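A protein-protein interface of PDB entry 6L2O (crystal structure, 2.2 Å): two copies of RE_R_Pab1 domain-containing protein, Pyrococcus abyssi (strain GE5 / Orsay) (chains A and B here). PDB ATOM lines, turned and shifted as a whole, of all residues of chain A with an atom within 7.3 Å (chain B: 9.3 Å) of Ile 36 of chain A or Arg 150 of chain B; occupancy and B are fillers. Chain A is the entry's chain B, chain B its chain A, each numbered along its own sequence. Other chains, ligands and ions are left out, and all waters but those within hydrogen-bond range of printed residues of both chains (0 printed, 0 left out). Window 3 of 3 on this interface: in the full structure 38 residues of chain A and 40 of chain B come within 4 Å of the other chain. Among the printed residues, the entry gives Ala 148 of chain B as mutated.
No position is printed for both chains. Of the 6 pairs that touch across the chains among the printed residues, none has its exchanged pair printed and touching as well.
Of chain B, only Arg 150 and Ala 151 come within 4 Å of Ile 36 of chain A. Of chain A, only Ile 36 and Pro 37 come within 4 Å of Arg 150 of chain B. No residue of chain B comes within 4 Å of Gly 35 of chain A. Of the printed residues of chain A, Ala 151 of chain B touches Ile 36 (3.7 Å). Printed residues of chain A within 4 Å of Gln 149 of chain B: Pro 37 (3.2 Å). Of the printed residues of chain B, Asn 32 of chain A touches Val 152. Of the printed residues of chain B, Val 34 of chain A touches His 147 (3.7 Å). Gly 153 of chain B touches none of the printed residues of chain A. The nearest residue of chain A that does not touch Arg 150 of chain B is Pro 21 of chain A (4.03 Å). The nearest printed residue of chain A that does not touch His 147 of chain B is Asn 32 of chain A (6.7 Å).
The side-chain amide oxygen (OE1) of Gln 149 of chain B lies close to the side-chain amide oxygen (OE1) of Gln 155 of chain B, at 3.0 Å. The backbone NH (N) of Ile 36 of chain A sits at hydrogen-bond distance from the backbone carbonyl oxygen (O) of Lys 29 of chain A (3.0 Å).
Printed residues of chain B that touch a printed residue of chain A: His 147, Gln 149, Arg 150, Ala 151 and Val 152. Hydrophobic or aromatic side chains of chain B within 4 Å of the printed part of chain A: His 147 and Val 152.
Among the printed residues, merely in contact across the chains: Asn 32 of chain A with Val 152 of chain B, Val 34 of chain A with His 147 of chain B, Ile 36 of chain A with Arg 150 of chain B, Ile 36 of chain A with Ala 151 of chain B, Pro 37 of chain A with Gln 149 of chain B and Pro 37 of chain A with Arg 150 of chain B.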
ATOM      1  N   PRO A  21      13.375 -15.438   7.136  1.00  0.00           N
ATOM      2  CA  PRO A  21      12.050 -14.852   6.883  1.00  0.00           C
ATOM      3  C   PRO A  21      10.949 -15.873   6.608  1.00  0.00           C
ATOM      4  O   PRO A  21       9.775 -15.482   6.592  1.00  0.00           O
ATOM      5  CB  PRO A  21      12.297 -13.955   5.663  1.00  0.00           C
ATOM      6  CG  PRO A  21      13.432 -14.600   4.954  1.00  0.00           C
ATOM      7  CD  PRO A  21      14.313 -15.186   6.028  1.00  0.00           C
ATOM      8  N   THR A  22      11.274 -17.156   6.399  1.00  0.00           N
ATOM      9  CA  THR A  22      10.233 -18.164   6.209  1.00  0.00           C
ATOM     10  C   THR A  22       9.748 -18.762   7.526  1.00  0.00           C
ATOM     11  O   THR A  22       8.724 -19.454   7.535  1.00  0.00           O
ATOM     12  CB  THR A  22      10.719 -19.307   5.295  1.00  0.00           C
ATOM     13  OG1 THR A  22      11.876 -19.938   5.858  1.00  0.00           O
ATOM     14  CG2 THR A  22      11.065 -18.791   3.904  1.00  0.00           C
ATOM     15  N   ARG A  26       9.968 -13.698  11.886  1.00  0.00           N
ATOM     16  CA  ARG A  26      10.426 -13.000  10.695  1.00  0.00           C
ATOM     17  C   ARG A  26      10.447 -11.501  10.948  1.00  0.00           C
ATOM     18  O   ARG A  26       9.604 -10.962  11.673  1.00  0.00           O
ATOM     19  CB  ARG A  26       9.536 -13.317   9.484  1.00  0.00           C
ATOM     20  CG  ARG A  26       8.055 -13.207   9.762  1.00  0.00           C
ATOM     21  CD  ARG A  26       7.227 -13.689   8.582  1.00  0.00           C
ATOM     22  NE  ARG A  26       7.190 -15.144   8.502  1.00  0.00           N
ATOM     23  CZ  ARG A  26       6.620 -15.826   7.515  1.00  0.00           C
ATOM     24  NH1 ARG A  26       6.028 -15.185   6.517  1.00  0.00           N
ATOM     25  NH2 ARG A  26       6.640 -17.153   7.528  1.00  0.00           N
ATOM     26  N   VAL A  27      11.430 -10.835  10.351  1.00  0.00           N
ATOM     27  CA  VAL A  27      11.555  -9.388  10.481  1.00  0.00           C
ATOM     28  C   VAL A  27      10.648  -8.719   9.459  1.00  0.00           C
ATOM     29  O   VAL A  27      10.607  -9.120   8.289  1.00  0.00           O
ATOM     30  CB  VAL A  27      13.015  -8.949  10.299  1.00  0.00           C
ATOM     31  CG1 VAL A  27      13.155  -7.451  10.557  1.00  0.00           C
ATOM     32  CG2 VAL A  27      13.920  -9.743  11.220  1.00  0.00           C
ATOM     33  N   LYS A  28       9.906  -7.708   9.897  1.00  0.00           N
ATOM     34  CA  LYS A  28       8.993  -6.993   9.021  1.00  0.00           C
ATOM     35  C   LYS A  28       9.131  -5.499   9.259  1.00  0.00           C
ATOM     36  O   LYS A  28       9.737  -5.050  10.236  1.00  0.00           O
ATOM     37  CB  LYS A  28       7.539  -7.432   9.228  1.00  0.00           C
ATOM     38  CG  LYS A  28       7.257  -8.847   8.763  1.00  0.00           C
ATOM     39  CD  LYS A  28       5.947  -8.919   8.007  1.00  0.00           C
ATOM     40  CE  LYS A  28       5.544 -10.359   7.755  1.00  0.00           C
ATOM     41  NZ  LYS A  28       4.641 -10.854   8.822  1.00  0.00           N
ATOM     42  N   LYS A  29       8.566  -4.724   8.341  1.00  0.00           N
ATOM     43  CA  LYS A  29       8.531  -3.282   8.494  1.00  0.00           C
ATOM     44  C   LYS A  29       7.199  -2.774   7.977  1.00  0.00           C
ATOM     45  O   LYS A  29       6.596  -3.370   7.079  1.00  0.00           O
ATOM     46  CB  LYS A  29       9.700  -2.600   7.763  1.00  0.00           C
ATOM     47  CG  LYS A  29       9.502  -2.424   6.269  1.00  0.00           C
ATOM     48  CD  LYS A  29      10.147  -1.137   5.777  1.00  0.00           C
ATOM     49  CE  LYS A  29       9.679   0.065   6.588  1.00  0.00           C
ATOM     50  NZ  LYS A  29       9.986   1.355   5.909  1.00  0.00           N
ATOM     51  N   ILE A  30       6.731  -1.678   8.569  1.00  0.00           N
ATOM     52  CA  ILE A  30       5.450  -1.094   8.187  1.00  0.00           C
ATOM     53  C   ILE A  30       5.675  -0.237   6.948  1.00  0.00           C
ATOM     54  O   ILE A  30       6.420   0.743   6.983  1.00  0.00           O
ATOM     55  CB  ILE A  30       4.834  -0.270   9.320  1.00  0.00           C
ATOM     56  CG1 ILE A  30       4.617  -1.138  10.558  1.00  0.00           C
ATOM     57  CG2 ILE A  30       3.517   0.319   8.857  1.00  0.00           C
ATOM     58  CD1 ILE A  30       3.509  -2.154  10.394  1.00  0.00           C
ATOM     59  N   GLU A  31       5.031  -0.613   5.849  1.00  0.00           N
ATOM     60  CA  GLU A  31       5.089   0.139   4.603  1.00  0.00           C
ATOM     61  C   GLU A  31       3.672   0.230   4.067  1.00  0.00           C
ATOM     62  O   GLU A  31       3.038  -0.798   3.813  1.00  0.00           O
ATOM     63  CB  GLU A  31       6.028  -0.530   3.589  1.00  0.00           C
ATOM     64  CG  GLU A  31       6.482   0.383   2.453  1.00  0.00           C
ATOM     65  CD  GLU A  31       7.581   1.356   2.864  1.00  0.00           C
ATOM     66  OE1 GLU A  31       8.101   1.239   3.994  1.00  0.00           O
ATOM     67  OE2 GLU A  31       7.924   2.241   2.049  1.00  0.00           O
ATOM     68  N   ASN A  32       3.169   1.452   3.928  1.00  0.00           N
ATOM     69  CA  ASN A  32       1.789   1.698   3.514  1.00  0.00           C
ATOM     70  C   ASN A  32       0.792   1.024   4.449  1.00  0.00           C
ATOM     71  O   ASN A  32      -0.295   0.627   4.026  1.00  0.00           O
ATOM     72  CB  ASN A  32       1.559   1.255   2.070  1.00  0.00           C
ATOM     73  CG  ASN A  32       0.479   2.056   1.379  1.00  0.00           C
ATOM     74  OD1 ASN A  32      -0.481   1.498   0.844  1.00  0.00           O
ATOM     75  ND2 ASN A  32       0.630   3.375   1.383  1.00  0.00           N
ATOM     76  N   GLY A  33       1.170   0.894   5.723  1.00  0.00           N
ATOM     77  CA  GLY A  33       0.304   0.348   6.747  1.00  0.00           C
ATOM     78  C   GLY A  33       0.244  -1.163   6.838  1.00  0.00           C
ATOM     79  O   GLY A  33      -0.561  -1.684   7.618  1.00  0.00           O
ATOM     80  N   VAL A  34       1.058  -1.888   6.070  1.00  0.00           N
ATOM     81  CA  VAL A  34       1.035  -3.346   6.083  1.00  0.00           C
ATOM     82  C   VAL A  34       2.427  -3.870   6.406  1.00  0.00           C
ATOM     83  O   VAL A  34       3.442  -3.252   6.067  1.00  0.00           O
ATOM     84  CB  VAL A  34       0.531  -3.934   4.745  1.00  0.00           C
ATOM     85  CG1 VAL A  34      -0.907  -3.524   4.492  1.00  0.00           C
ATOM     86  CG2 VAL A  34       1.425  -3.504   3.595  1.00  0.00           C
ATOM     87  N   GLY A  35       2.468  -5.024   7.068  1.00  0.00           N
ATOM     88  CA  GLY A  35       3.732  -5.686   7.340  1.00  0.00           C
ATOM     89  C   GLY A  35       4.328  -6.272   6.068  1.00  0.00           C
ATOM     90  O   GLY A  35       3.663  -7.048   5.365  1.00  0.00           O
ATOM     91  N   ILE A  36       5.572  -5.913   5.769  1.00  0.00           N
ATOM     92  CA  ILE A  36       6.264  -6.350   4.560  1.00  0.00           C
ATOM     93  C   ILE A  36       7.518  -7.093   4.997  1.00  0.00           C
ATOM     94  O   ILE A  36       8.239  -6.608   5.866  1.00  0.00           O
ATOM     95  CB  ILE A  36       6.638  -5.171   3.643  1.00  0.00           C
ATOM     96  CG1 ILE A  36       5.378  -4.515   3.079  1.00  0.00           C
ATOM     97  CG2 ILE A  36       7.563  -5.620   2.522  1.00  0.00           C
ATOM     98  CD1 ILE A  36       4.522  -5.450   2.269  1.00  0.00           C
ATOM     99  N   PRO A  37       7.808  -8.273   4.441  1.00  0.00           N
ATOM    100  CA  PRO A  37       9.078  -8.936   4.763  1.00  0.00           C
ATOM    101  C   PRO A  37      10.260  -8.042   4.418  1.00  0.00           C
ATOM    102  O   PRO A  37      10.246  -7.319   3.419  1.00  0.00           O
ATOM    103  CB  PRO A  37       9.051 -10.201   3.893  1.00  0.00           C
ATOM    104  CG  PRO A  37       7.608 -10.455   3.630  1.00  0.00           C
ATOM    105  CD  PRO A  37       6.962  -9.094   3.559  1.00  0.00           C
ATOM    106  N   VAL A  38      11.284  -8.080   5.269  1.00  0.00           N
ATOM    107  CA  VAL A  38      12.507  -7.310   5.075  1.00  0.00           C
ATOM    108  C   VAL A  38      13.639  -8.277   4.766  1.00  0.00           C
ATOM    109  O   VAL A  38      13.774  -9.315   5.424  1.00  0.00           O
ATOM    110  CB  VAL A  38      12.851  -6.457   6.310  1.00  0.00           C
ATOM    111  CG1 VAL A  38      14.065  -5.588   6.027  1.00  0.00           C
ATOM    112  CG2 VAL A  38      11.660  -5.600   6.736  1.00  0.00           C
ATOM    113  N   SER A  39      14.461  -7.930   3.774  1.00  0.00           N
ATOM    114  CA  SER A  39      15.676  -8.685   3.471  1.00  0.00           C
ATOM    115  C   SER A  39      16.788  -8.173   4.377  1.00  0.00           C
ATOM    116  O   SER A  39      17.555  -7.279   4.017  1.00  0.00           O
ATOM    117  CB  SER A  39      16.048  -8.547   2.000  1.00  0.00           C
ATOM    118  OG  SER A  39      15.037  -9.080   1.162  1.00  0.00           O
ATOM    119  N   TYR A  54      10.175  -0.911  11.900  1.00  0.00           N
ATOM    120  CA  TYR A  54      10.624  -2.290  11.774  1.00  0.00           C
ATOM    121  C   TYR A  54      10.291  -3.072  13.037  1.00  0.00           C
ATOM    122  O   TYR A  54      10.414  -2.556  14.153  1.00  0.00           O
ATOM    123  CB  TYR A  54      12.131  -2.339  11.520  1.00  0.00           C
ATOM    124  CG  TYR A  54      12.558  -1.857  10.152  1.00  0.00           C
ATOM    125  CD1 TYR A  54      12.501  -0.510   9.816  1.00  0.00           C
ATOM    126  CD2 TYR A  54      13.033  -2.749   9.199  1.00  0.00           C
ATOM    127  CE1 TYR A  54      12.895  -0.069   8.565  1.00  0.00           C
ATOM    128  CE2 TYR A  54      13.433  -2.316   7.949  1.00  0.00           C
ATOM    129  CZ  TYR A  54      13.364  -0.976   7.639  1.00  0.00           C
ATOM    130  OH  TYR A  54      13.759  -0.545   6.394  1.00  0.00           O
ATOM    131  N   TYR A  55       9.882  -4.326  12.862  1.00  0.00           N
ATOM    132  CA  TYR A  55       9.553  -5.153  14.011  1.00  0.00           C
ATOM    133  C   TYR A  55       9.795  -6.615  13.676  1.00  0.00           C
ATOM    134  O   TYR A  55       9.928  -6.994  12.511  1.00  0.00           O
ATOM    135  CB  TYR A  55       8.104  -4.936  14.467  1.00  0.00           C
ATOM    136  CG  TYR A  55       7.057  -5.313  13.444  1.00  0.00           C
ATOM    137  CD1 TYR A  55       6.694  -4.430  12.434  1.00  0.00           C
ATOM    138  CD2 TYR A  55       6.416  -6.549  13.496  1.00  0.00           C
ATOM    139  CE1 TYR A  55       5.732  -4.770  11.494  1.00  0.00           C
ATOM    140  CE2 TYR A  55       5.452  -6.897  12.563  1.00  0.00           C
ATOM    141  CZ  TYR A  55       5.116  -6.004  11.565  1.00  0.00           C
ATOM    142  OH  TYR A  55       4.155  -6.335  10.636  1.00  0.00           O
ATOM    143  N   HIS B 147      -3.196  -9.487  -0.287  1.00  0.00           N
ATOM    144  CA  HIS B 147      -2.083  -8.548  -0.290  1.00  0.00           C
ATOM    145  C   HIS B 147      -0.879  -9.145  -1.007  1.00  0.00           C
ATOM    146  O   HIS B 147      -0.576 -10.334  -0.867  1.00  0.00           O
ATOM    147  CB  HIS B 147      -1.697  -8.171   1.140  1.00  0.00           C
ATOM    148  CG  HIS B 147      -2.548  -7.089   1.727  1.00  0.00           C
ATOM    149  ND1 HIS B 147      -2.386  -5.758   1.408  1.00  0.00           N
ATOM    150  CD2 HIS B 147      -3.577  -7.143   2.607  1.00  0.00           C
ATOM    151  CE1 HIS B 147      -3.282  -5.040   2.061  1.00  0.00           C
ATOM    152  NE2 HIS B 147      -4.015  -5.855   2.796  1.00  0.00           N
ATOM    153  N   ALA B 148      -0.195  -8.311  -1.787  1.00  0.00           N
ATOM    154  CA  ALA B 148       1.085  -8.705  -2.351  1.00  0.00           C
ATOM    155  C   ALA B 148       2.061  -9.022  -1.227  1.00  0.00           C
ATOM    156  O   ALA B 148       2.228  -8.234  -0.290  1.00  0.00           O
ATOM    157  CB  ALA B 148       1.637  -7.596  -3.244  1.00  0.00           C
ATOM    158  N   GLN B 149       2.704 -10.185  -1.326  1.00  0.00           N
ATOM    159  CA  GLN B 149       3.509 -10.705  -0.224  1.00  0.00           C
ATOM    160  C   GLN B 149       4.760  -9.863   0.000  1.00  0.00           C
ATOM    161  O   GLN B 149       4.987  -9.340   1.098  1.00  0.00           O
ATOM    162  CB  GLN B 149       3.885 -12.163  -0.503  1.00  0.00           C
ATOM    163  CG  GLN B 149       2.753 -13.027  -1.065  1.00  0.00           C
ATOM    164  CD  GLN B 149       2.510 -12.817  -2.553  1.00  0.00           C
ATOM    165  OE1 GLN B 149       2.443 -11.683  -3.031  1.00  0.00           O
ATOM    166  NE2 GLN B 149       2.373 -13.914  -3.291  1.00  0.00           N
ATOM    167  N   ARG B 150       5.586  -9.724  -1.033  1.00  0.00           N
ATOM    168  CA  ARG B 150       6.891  -9.087  -0.913  1.00  0.00           C
ATOM    169  C   ARG B 150       6.867  -7.591  -1.205  1.00  0.00           C
ATOM    170  O   ARG B 150       7.918  -6.945  -1.130  1.00  0.00           O
ATOM    171  CB  ARG B 150       7.892  -9.779  -1.847  1.00  0.00           C
ATOM    172  CG  ARG B 150       8.946 -10.605  -1.130  1.00  0.00           C
ATOM    173  CD  ARG B 150       8.325 -11.725  -0.308  1.00  0.00           C
ATOM    174  NE  ARG B 150       9.232 -12.184   0.741  1.00  0.00           N
ATOM    175  CZ  ARG B 150       9.011 -13.243   1.515  1.00  0.00           C
ATOM    176  NH1 ARG B 150       7.906 -13.961   1.358  1.00  0.00           N
ATOM    177  NH2 ARG B 150       9.895 -13.582   2.444  1.00  0.00           N
ATOM    178  N   ALA B 151       5.709  -7.022  -1.526  1.00  0.00           N
ATOM    179  CA  ALA B 151       5.632  -5.613  -1.878  1.00  0.00           C
ATOM    180  C   ALA B 151       4.244  -5.090  -1.540  1.00  0.00           C
ATOM    181  O   ALA B 151       3.335  -5.851  -1.203  1.00  0.00           O
ATOM    182  CB  ALA B 151       5.959  -5.391  -3.359  1.00  0.00           C
ATOM    183  N   VAL B 152       4.089  -3.769  -1.633  1.00  0.00           N
ATOM    184  CA  VAL B 152       2.787  -3.160  -1.404  1.00  0.00           C
ATOM    185  C   VAL B 152       1.905  -3.360  -2.633  1.00  0.00           C
ATOM    186  O   VAL B 152       2.376  -3.620  -3.743  1.00  0.00           O
ATOM    187  CB  VAL B 152       2.915  -1.669  -1.047  1.00  0.00           C
ATOM    188  CG1 VAL B 152       3.125  -0.834  -2.300  1.00  0.00           C
ATOM    189  CG2 VAL B 152       1.683  -1.205  -0.299  1.00  0.00           C
ATOM    190  N   GLY B 153       0.602  -3.237  -2.422  1.00  0.00           N
ATOM    191  CA  GLY B 153      -0.369  -3.457  -3.471  1.00  0.00           C
ATOM    192  C   GLY B 153      -1.048  -4.803  -3.324  1.00  0.00           C
ATOM    193  O   GLY B 153      -0.766  -5.595  -2.420  1.00  0.00           O
ATOM    194  N   TYR B 154      -1.966  -5.058  -4.246  1.00  0.00           N
ATOM    195  CA  TYR B 154      -2.746  -6.283  -4.240  1.00  0.00           C
ATOM    196  C   TYR B 154      -2.284  -7.203  -5.361  1.00  0.00           C
ATOM    197  O   TYR B 154      -1.691  -6.763  -6.349  1.00  0.00           O
ATOM    198  CB  TYR B 154      -4.242  -5.988  -4.397  1.00  0.00           C
ATOM    199  CG  TYR B 154      -4.794  -4.991  -3.398  1.00  0.00           C
ATOM    200  CD1 TYR B 154      -5.302  -3.768  -3.815  1.00  0.00           C
ATOM    201  CD2 TYR B 154      -4.811  -5.274  -2.037  1.00  0.00           C
ATOM    202  CE1 TYR B 154      -5.814  -2.857  -2.906  1.00  0.00           C
ATOM    203  CE2 TYR B 154      -5.312  -4.363  -1.120  1.00  0.00           C
ATOM    204  CZ  TYR B 154      -5.818  -3.161  -1.563  1.00  0.00           C
ATOM    205  OH  TYR B 154      -6.325  -2.253  -0.665  1.00  0.00           O
ATOM    206  N   GLN B 155      -2.545  -8.491  -5.182  1.00  0.00           N
ATOM    207  CA  GLN B 155      -2.451  -9.470  -6.251  1.00  0.00           C
ATOM    208  C   GLN B 155      -3.718 -10.309  -6.232  1.00  0.00           C
ATOM    209  O   GLN B 155      -4.234 -10.647  -5.162  1.00  0.00           O
ATOM    210  CB  GLN B 155      -1.209 -10.362  -6.108  1.00  0.00           C
ATOM    211  CG  GLN B 155      -1.137 -11.134  -4.810  1.00  0.00           C
ATOM    212  CD  GLN B 155      -0.147 -12.283  -4.870  1.00  0.00           C
ATOM    213  OE1 GLN B 155       0.886 -12.195  -5.538  1.00  0.00           O
ATOM    214  NE2 GLN B 155      -0.460 -13.370  -4.173  1.00  0.00           N
